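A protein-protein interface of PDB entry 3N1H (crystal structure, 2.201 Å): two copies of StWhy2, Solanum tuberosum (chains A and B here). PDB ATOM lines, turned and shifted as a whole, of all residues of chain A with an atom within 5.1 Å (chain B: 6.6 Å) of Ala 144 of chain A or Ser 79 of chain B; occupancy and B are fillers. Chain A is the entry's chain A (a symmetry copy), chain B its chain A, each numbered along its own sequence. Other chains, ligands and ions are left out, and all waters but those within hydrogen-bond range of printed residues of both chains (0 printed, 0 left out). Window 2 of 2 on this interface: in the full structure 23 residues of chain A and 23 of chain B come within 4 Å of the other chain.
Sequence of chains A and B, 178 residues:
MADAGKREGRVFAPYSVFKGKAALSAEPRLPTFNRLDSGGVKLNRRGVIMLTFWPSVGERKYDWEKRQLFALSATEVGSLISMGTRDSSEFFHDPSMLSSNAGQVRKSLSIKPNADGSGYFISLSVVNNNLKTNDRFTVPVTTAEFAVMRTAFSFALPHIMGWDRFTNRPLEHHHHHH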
ATOM      1  N   TYR A  15     -35.942 -13.694 -20.365  1.00  0.00           N
ATOM      2  CA  TYR A  15     -34.776 -12.821 -20.443  1.00  0.00           C
ATOM      3  C   TYR A  15     -33.567 -13.723 -20.538  1.00  0.00           C
ATOM      4  O   TYR A  15     -33.379 -14.589 -19.712  1.00  0.00           O
ATOM      5  CB  TYR A  15     -34.656 -11.897 -19.228  1.00  0.00           C
ATOM      6  CG  TYR A  15     -33.357 -11.104 -19.185  1.00  0.00           C
ATOM      7  CD1 TYR A  15     -33.052 -10.158 -20.167  1.00  0.00           C
ATOM      8  CD2 TYR A  15     -32.436 -11.303 -18.168  1.00  0.00           C
ATOM      9  CE1 TYR A  15     -31.862  -9.434 -20.125  1.00  0.00           C
ATOM     10  CE2 TYR A  15     -31.229 -10.588 -18.122  1.00  0.00           C
ATOM     11  CZ  TYR A  15     -30.946  -9.659 -19.088  1.00  0.00           C
ATOM     12  OH  TYR A  15     -29.756  -8.949 -19.011  1.00  0.00           O
ATOM     13  N   THR A 142     -22.928 -10.042 -15.880  1.00  0.00           N
ATOM     14  CA  THR A 142     -22.348  -8.764 -15.503  1.00  0.00           C
ATOM     15  C   THR A 142     -23.246  -8.101 -14.492  1.00  0.00           C
ATOM     16  O   THR A 142     -24.391  -8.532 -14.260  1.00  0.00           O
ATOM     17  CB  THR A 142     -22.280  -7.819 -16.705  1.00  0.00           C
ATOM     18  OG1 THR A 142     -23.612  -7.502 -17.116  1.00  0.00           O
ATOM     19  CG2 THR A 142     -21.571  -8.477 -17.851  1.00  0.00           C
ATOM     20  N   THR A 143     -22.742  -7.018 -13.922  1.00  0.00           N
ATOM     21  CA  THR A 143     -23.539  -6.219 -13.003  1.00  0.00           C
ATOM     22  C   THR A 143     -24.875  -5.717 -13.604  1.00  0.00           C
ATOM     23  O   THR A 143     -25.913  -5.737 -12.926  1.00  0.00           O
ATOM     24  CB  THR A 143     -22.706  -5.043 -12.469  1.00  0.00           C
ATOM     25  OG1 THR A 143     -21.624  -5.572 -11.708  1.00  0.00           O
ATOM     26  CG2 THR A 143     -23.552  -4.094 -11.575  1.00  0.00           C
ATOM     27  N   ALA A 144     -24.832  -5.263 -14.860  1.00  0.00           N
ATOM     28  CA  ALA A 144     -26.011  -4.738 -15.540  1.00  0.00           C
ATOM     29  C   ALA A 144     -27.016  -5.850 -15.812  1.00  0.00           C
ATOM     30  O   ALA A 144     -28.222  -5.629 -15.691  1.00  0.00           O
ATOM     31  CB  ALA A 144     -25.628  -4.047 -16.872  1.00  0.00           C
ATOM     32  N   GLU A 145     -26.506  -7.016 -16.221  1.00  0.00           N
ATOM     33  CA  GLU A 145     -27.317  -8.194 -16.459  1.00  0.00           C
ATOM     34  C   GLU A 145     -28.004  -8.607 -15.179  1.00  0.00           C
ATOM     35  O   GLU A 145     -29.176  -8.892 -15.172  1.00  0.00           O
ATOM     36  CB  GLU A 145     -26.471  -9.336 -17.033  1.00  0.00           C
ATOM     37  CG  GLU A 145     -26.377  -9.249 -18.595  1.00  0.00           C
ATOM     38  CD  GLU A 145     -25.246 -10.100 -19.196  1.00  0.00           C
ATOM     39  OE1 GLU A 145     -24.379 -10.598 -18.436  1.00  0.00           O
ATOM     40  OE2 GLU A 145     -25.223 -10.251 -20.441  1.00  0.00           O
ATOM     41  N   PHE A 146     -27.284  -8.572 -14.075  1.00  0.00           N
ATOM     42  CA  PHE A 146     -27.874  -8.967 -12.823  1.00  0.00           C
ATOM     43  C   PHE A 146     -28.810  -7.876 -12.328  1.00  0.00           C
ATOM     44  O   PHE A 146     -29.800  -8.157 -11.655  1.00  0.00           O
ATOM     45  CB  PHE A 146     -26.774  -9.272 -11.795  1.00  0.00           C
ATOM     46  CG  PHE A 146     -27.266  -9.979 -10.568  1.00  0.00           C
ATOM     47  CD1 PHE A 146     -27.556 -11.332 -10.607  1.00  0.00           C
ATOM     48  CD2 PHE A 146     -27.439  -9.290  -9.369  1.00  0.00           C
ATOM     49  CE1 PHE A 146     -28.013 -12.002  -9.481  1.00  0.00           C
ATOM     50  CE2 PHE A 146     -27.889  -9.959  -8.216  1.00  0.00           C
ATOM     51  CZ  PHE A 146     -28.176 -11.325  -8.278  1.00  0.00           C
ATOM     52  N   ALA A 147     -28.508  -6.617 -12.655  1.00  0.00           N
ATOM     53  CA  ALA A 147     -29.436  -5.556 -12.276  1.00  0.00           C
ATOM     54  C   ALA A 147     -30.757  -5.726 -13.027  1.00  0.00           C
ATOM     55  O   ALA A 147     -31.813  -5.416 -12.480  1.00  0.00           O
ATOM     56  CB  ALA A 147     -28.851  -4.228 -12.567  1.00  0.00           C
ATOM     57  N   VAL A 148     -30.713  -6.201 -14.284  1.00  0.00           N
ATOM     58  CA  VAL A 148     -31.964  -6.487 -15.022  1.00  0.00           C
ATOM     59  C   VAL A 148     -32.691  -7.615 -14.271  1.00  0.00           C
ATOM     60  O   VAL A 148     -33.878  -7.507 -13.967  1.00  0.00           O
ATOM     61  CB  VAL A 148     -31.740  -6.920 -16.525  1.00  0.00           C
ATOM     62  CG1 VAL A 148     -33.063  -7.385 -17.145  1.00  0.00           C
ATOM     63  CG2 VAL A 148     -31.138  -5.800 -17.358  1.00  0.00           C
ATOM     64  N   ALA B  74     -32.649  -3.642 -22.871  1.00  0.00           N
ATOM     65  CA  ALA B  74     -32.961  -3.894 -21.451  1.00  0.00           C
ATOM     66  C   ALA B  74     -31.678  -3.865 -20.633  1.00  0.00           C
ATOM     67  O   ALA B  74     -31.599  -3.304 -19.510  1.00  0.00           O
ATOM     68  CB  ALA B  74     -33.655  -5.218 -21.291  1.00  0.00           C
ATOM     69  N   THR B  75     -30.644  -4.449 -21.202  1.00  0.00           N
ATOM     70  CA  THR B  75     -29.369  -4.542 -20.483  1.00  0.00           C
ATOM     71  C   THR B  75     -28.707  -3.163 -20.280  1.00  0.00           C
ATOM     72  O   THR B  75     -28.152  -2.876 -19.203  1.00  0.00           O
ATOM     73  CB  THR B  75     -28.408  -5.556 -21.146  1.00  0.00           C
ATOM     74  OG1 THR B  75     -29.038  -6.843 -21.191  1.00  0.00           O
ATOM     75  CG2 THR B  75     -27.168  -5.698 -20.332  1.00  0.00           C
ATOM     76  N   GLU B  76     -28.775  -2.312 -21.304  1.00  0.00           N
ATOM     77  CA  GLU B  76     -28.302  -0.933 -21.191  1.00  0.00           C
ATOM     78  C   GLU B  76     -29.113  -0.145 -20.155  1.00  0.00           C
ATOM     79  O   GLU B  76     -28.550   0.641 -19.406  1.00  0.00           O
ATOM     80  CB  GLU B  76     -28.296  -0.245 -22.591  1.00  0.00           C
ATOM     81  CG  GLU B  76     -27.194  -0.847 -23.549  1.00  0.00           C
ATOM     82  CD  GLU B  76     -27.303  -0.412 -25.043  1.00  0.00           C
ATOM     83  OE1 GLU B  76     -28.425  -0.064 -25.508  1.00  0.00           O
ATOM     84  OE2 GLU B  76     -26.264  -0.457 -25.770  1.00  0.00           O
ATOM     85  N   VAL B  77     -30.437  -0.327 -20.135  1.00  0.00           N
ATOM     86  CA  VAL B  77     -31.275   0.255 -19.092  1.00  0.00           C
ATOM     87  C   VAL B  77     -30.818  -0.253 -17.740  1.00  0.00           C
ATOM     88  O   VAL B  77     -30.656   0.522 -16.792  1.00  0.00           O
ATOM     89  CB  VAL B  77     -32.733  -0.152 -19.237  1.00  0.00           C
ATOM     90  CG1 VAL B  77     -33.535   0.334 -17.990  1.00  0.00           C
ATOM     91  CG2 VAL B  77     -33.300   0.420 -20.512  1.00  0.00           C
ATOM     92  N   GLY B  78     -30.584  -1.564 -17.666  1.00  0.00           N
ATOM     93  CA  GLY B  78     -30.083  -2.188 -16.457  1.00  0.00           C
ATOM     94  C   GLY B  78     -28.849  -1.473 -15.962  1.00  0.00           C
ATOM     95  O   GLY B  78     -28.659  -1.241 -14.759  1.00  0.00           O
ATOM     96  N   SER B  79     -28.003  -1.100 -16.901  1.00  0.00           N
ATOM     97  CA  SER B  79     -26.751  -0.468 -16.560  1.00  0.00           C
ATOM     98  C   SER B  79     -26.969   0.984 -16.104  1.00  0.00           C
ATOM     99  O   SER B  79     -26.330   1.457 -15.201  1.00  0.00           O
ATOM    100  CB  SER B  79     -25.794  -0.614 -17.740  1.00  0.00           C
ATOM    101  OG  SER B  79     -24.901   0.458 -17.817  1.00  0.00           O
ATOM    102  N   LEU B  80     -27.935   1.665 -16.684  1.00  0.00           N
ATOM    103  CA  LEU B  80     -28.243   3.053 -16.317  1.00  0.00           C
ATOM    104  C   LEU B  80     -28.838   3.160 -14.894  1.00  0.00           C
ATOM    105  O   LEU B  80     -28.493   4.056 -14.129  1.00  0.00           O
ATOM    106  CB  LEU B  80     -29.260   3.574 -17.338  1.00  0.00           C
ATOM    107  CG  LEU B  80     -29.451   5.059 -17.592  1.00  0.00           C
ATOM    108  CD1 LEU B  80     -29.807   5.308 -19.067  1.00  0.00           C
ATOM    109  CD2 LEU B  80     -30.520   5.586 -16.651  1.00  0.00           C
ATOM    110  N   ILE B  81     -29.741   2.245 -14.545  1.00  0.00           N
ATOM    111  CA  ILE B  81     -30.490   2.365 -13.287  1.00  0.00           C
ATOM    112  C   ILE B  81     -29.635   1.924 -12.103  1.00  0.00           C
ATOM    113  O   ILE B  81     -29.924   2.226 -10.937  1.00  0.00           O
ATOM    114  CB  ILE B  81     -31.836   1.587 -13.302  1.00  0.00           C
ATOM    115  CG1 ILE B  81     -31.574   0.100 -13.395  1.00  0.00           C
ATOM    116  CG2 ILE B  81     -32.751   2.058 -14.459  1.00  0.00           C
ATOM    117  CD1 ILE B  81     -32.862  -0.735 -13.481  1.00  0.00           C
ATOM    118  N   SER B  82     -28.561   1.231 -12.426  1.00  0.00           N
ATOM    119  CA  SER B  82     -27.658   0.788 -11.407  1.00  0.00           C
ATOM    120  C   SER B  82     -26.396   1.672 -11.428  1.00  0.00           C
ATOM    121  O   SER B  82     -25.347   1.281 -10.944  1.00  0.00           O
ATOM    122  CB  SER B  82     -27.373  -0.723 -11.568  1.00  0.00           C
ATOM    123  OG  SER B  82     -26.536  -1.013 -12.667  1.00  0.00           O
ATOM    124  N   MET B  83     -26.520   2.884 -11.967  1.00  0.00           N
ATOM    125  CA  MET B  83     -25.418   3.838 -11.938  1.00  0.00           C
ATOM    126  C   MET B  83     -25.450   4.602 -10.630  1.00  0.00           C
ATOM    127  O   MET B  83     -26.488   5.131 -10.242  1.00  0.00           O
ATOM    128  CB  MET B  83     -25.512   4.841 -13.094  1.00  0.00           C
ATOM    129  CG  MET B  83     -24.823   4.389 -14.322  1.00  0.00           C
ATOM    130  SD  MET B  83     -24.935   5.681 -15.580  1.00  0.00           S
ATOM    131  CE  MET B  83     -23.487   6.669 -15.184  1.00  0.00           C
ATOM    132  N   GLY B  84     -24.302   4.672  -9.974  1.00  0.00           N
ATOM    133  CA  GLY B  84     -24.158   5.476  -8.774  1.00  0.00           C
ATOM    134  C   GLY B  84     -23.760   6.898  -9.126  1.00  0.00           C
ATOM    135  O   GLY B  84     -23.399   7.182 -10.278  1.00  0.00           O
ATOM    136  N   SER B  88     -19.996   6.300 -14.462  1.00  0.00           N
ATOM    137  CA  SER B  88     -19.927   6.734 -15.838  1.00  0.00           C
ATOM    138  C   SER B  88     -20.283   5.522 -16.744  1.00  0.00           C
ATOM    139  O   SER B  88     -20.040   4.380 -16.368  1.00  0.00           O
ATOM    140  CB  SER B  88     -18.496   7.201 -16.058  1.00  0.00           C
ATOM    141  OG  SER B  88     -18.262   7.653 -17.365  1.00  0.00           O
ATOM    142  N   SER B  89     -20.899   5.734 -17.905  1.00  0.00           N
ATOM    143  CA  SER B  89     -20.974   4.653 -18.911  1.00  0.00           C
ATOM    144  C   SER B  89     -20.870   5.150 -20.339  1.00  0.00           C
ATOM    145  O   SER B  89     -20.981   6.342 -20.618  1.00  0.00           O
ATOM    146  CB  SER B  89     -22.218   3.770 -18.770  1.00  0.00           C
ATOM    147  OG  SER B  89     -23.325   4.498 -18.285  1.00  0.00           O
ATOM    148  N   PHE B  91     -22.023   3.486 -24.331  1.00  0.00           N
ATOM    149  CA  PHE B  91     -22.582   2.381 -25.100  1.00  0.00           C
ATOM    150  C   PHE B  91     -22.225   2.591 -26.590  1.00  0.00           C
ATOM    151  O   PHE B  91     -22.291   3.717 -27.071  1.00  0.00           O
ATOM    152  CB  PHE B  91     -24.114   2.319 -24.912  1.00  0.00           C
ATOM    153  CG  PHE B  91     -24.585   2.288 -23.468  1.00  0.00           C
ATOM    154  CD1 PHE B  91     -24.138   1.322 -22.569  1.00  0.00           C
ATOM    155  CD2 PHE B  91     -25.529   3.200 -23.013  1.00  0.00           C
ATOM    156  CE1 PHE B  91     -24.614   1.292 -21.223  1.00  0.00           C
ATOM    157  CE2 PHE B  91     -26.013   3.169 -21.677  1.00  0.00           C
ATOM    158  CZ  PHE B  91     -25.546   2.226 -20.791  1.00  0.00           C
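The side-chain hydroxyl of Tyr 15 of chain A is in hydrogen-bond range of the side-chain hydroxyl of Thr 75 of chain B, at 3.1 Å.
The backbone NH (N) of Ala 144 of chain A sits close to the side-chain hydroxyl (OG1) of Thr 142 of chain A, 3.4 Å away.
O of Gly 78 of chain B lies within hydrogen-bond range of OG of Ser 82 of chain B.
Among the printed residues, merely in contact across the chains: Ala 144 of chain A with Thr 75 of chain B, Ala 144 of chain A with Gly 78 of chain B, Ala 144 of chain A with Ser 79 of chain B, Ala 147 of chain A with Gly 78 of chain B, Ala 147 of chain A with Ser 82 of chain B, Val 148 of chain A with Ala 74 of chain B, Val 148 of chain A with Thr 75 of chain B and Val 148 of chain A with Gly 78 of chain B.
Of the printed residues of chain B, Ala 144 of chain A touches Thr 75 (3.6 Å), Gly 78 (3.99 Å) and Ser 79 (3.5 Å).
Ser 79 of chain B touches one residue of chain A.
Of the printed residues of chain A, Thr 75 of chain B touches Tyr 15 (3.1 Å), Ala 144 (3.6 Å) and Val 148 (3.8 Å).
Printed residues of chain B within 4 Å of Ala 147 of chain A: Gly 78 (3.7 Å) and Ser 82 (3.9 Å).
The nearest printed residue of chain B that does not touch Ala 147 of chain A is Ile 81 of chain B (4.9 Å).
Printed residues of chain B that touch a printed residue of chain A: Ala 74, Thr 75, Gly 78, Ser 79 and Ser 82.
Of the 8 printed residues of chain A, 4 touch a printed residue of chain B.
Hydrophobic or aromatic side chains of chain A that line the printed part of chain B: Tyr 15, Ala 144, Ala 147 and Val 148.
Along chain A the printed residues that touch a printed residue of chain B span positions 15 to 148.
Among the printed residues, no Asp or Glu carboxylate lies within 4 Å of a Lys or Arg side-chain nitrogen of the other chain.
No position is printed for both chains.
Of the 9 pairs that touch across the chains among the printed residues, none has its exchanged pair printed and touching as well.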
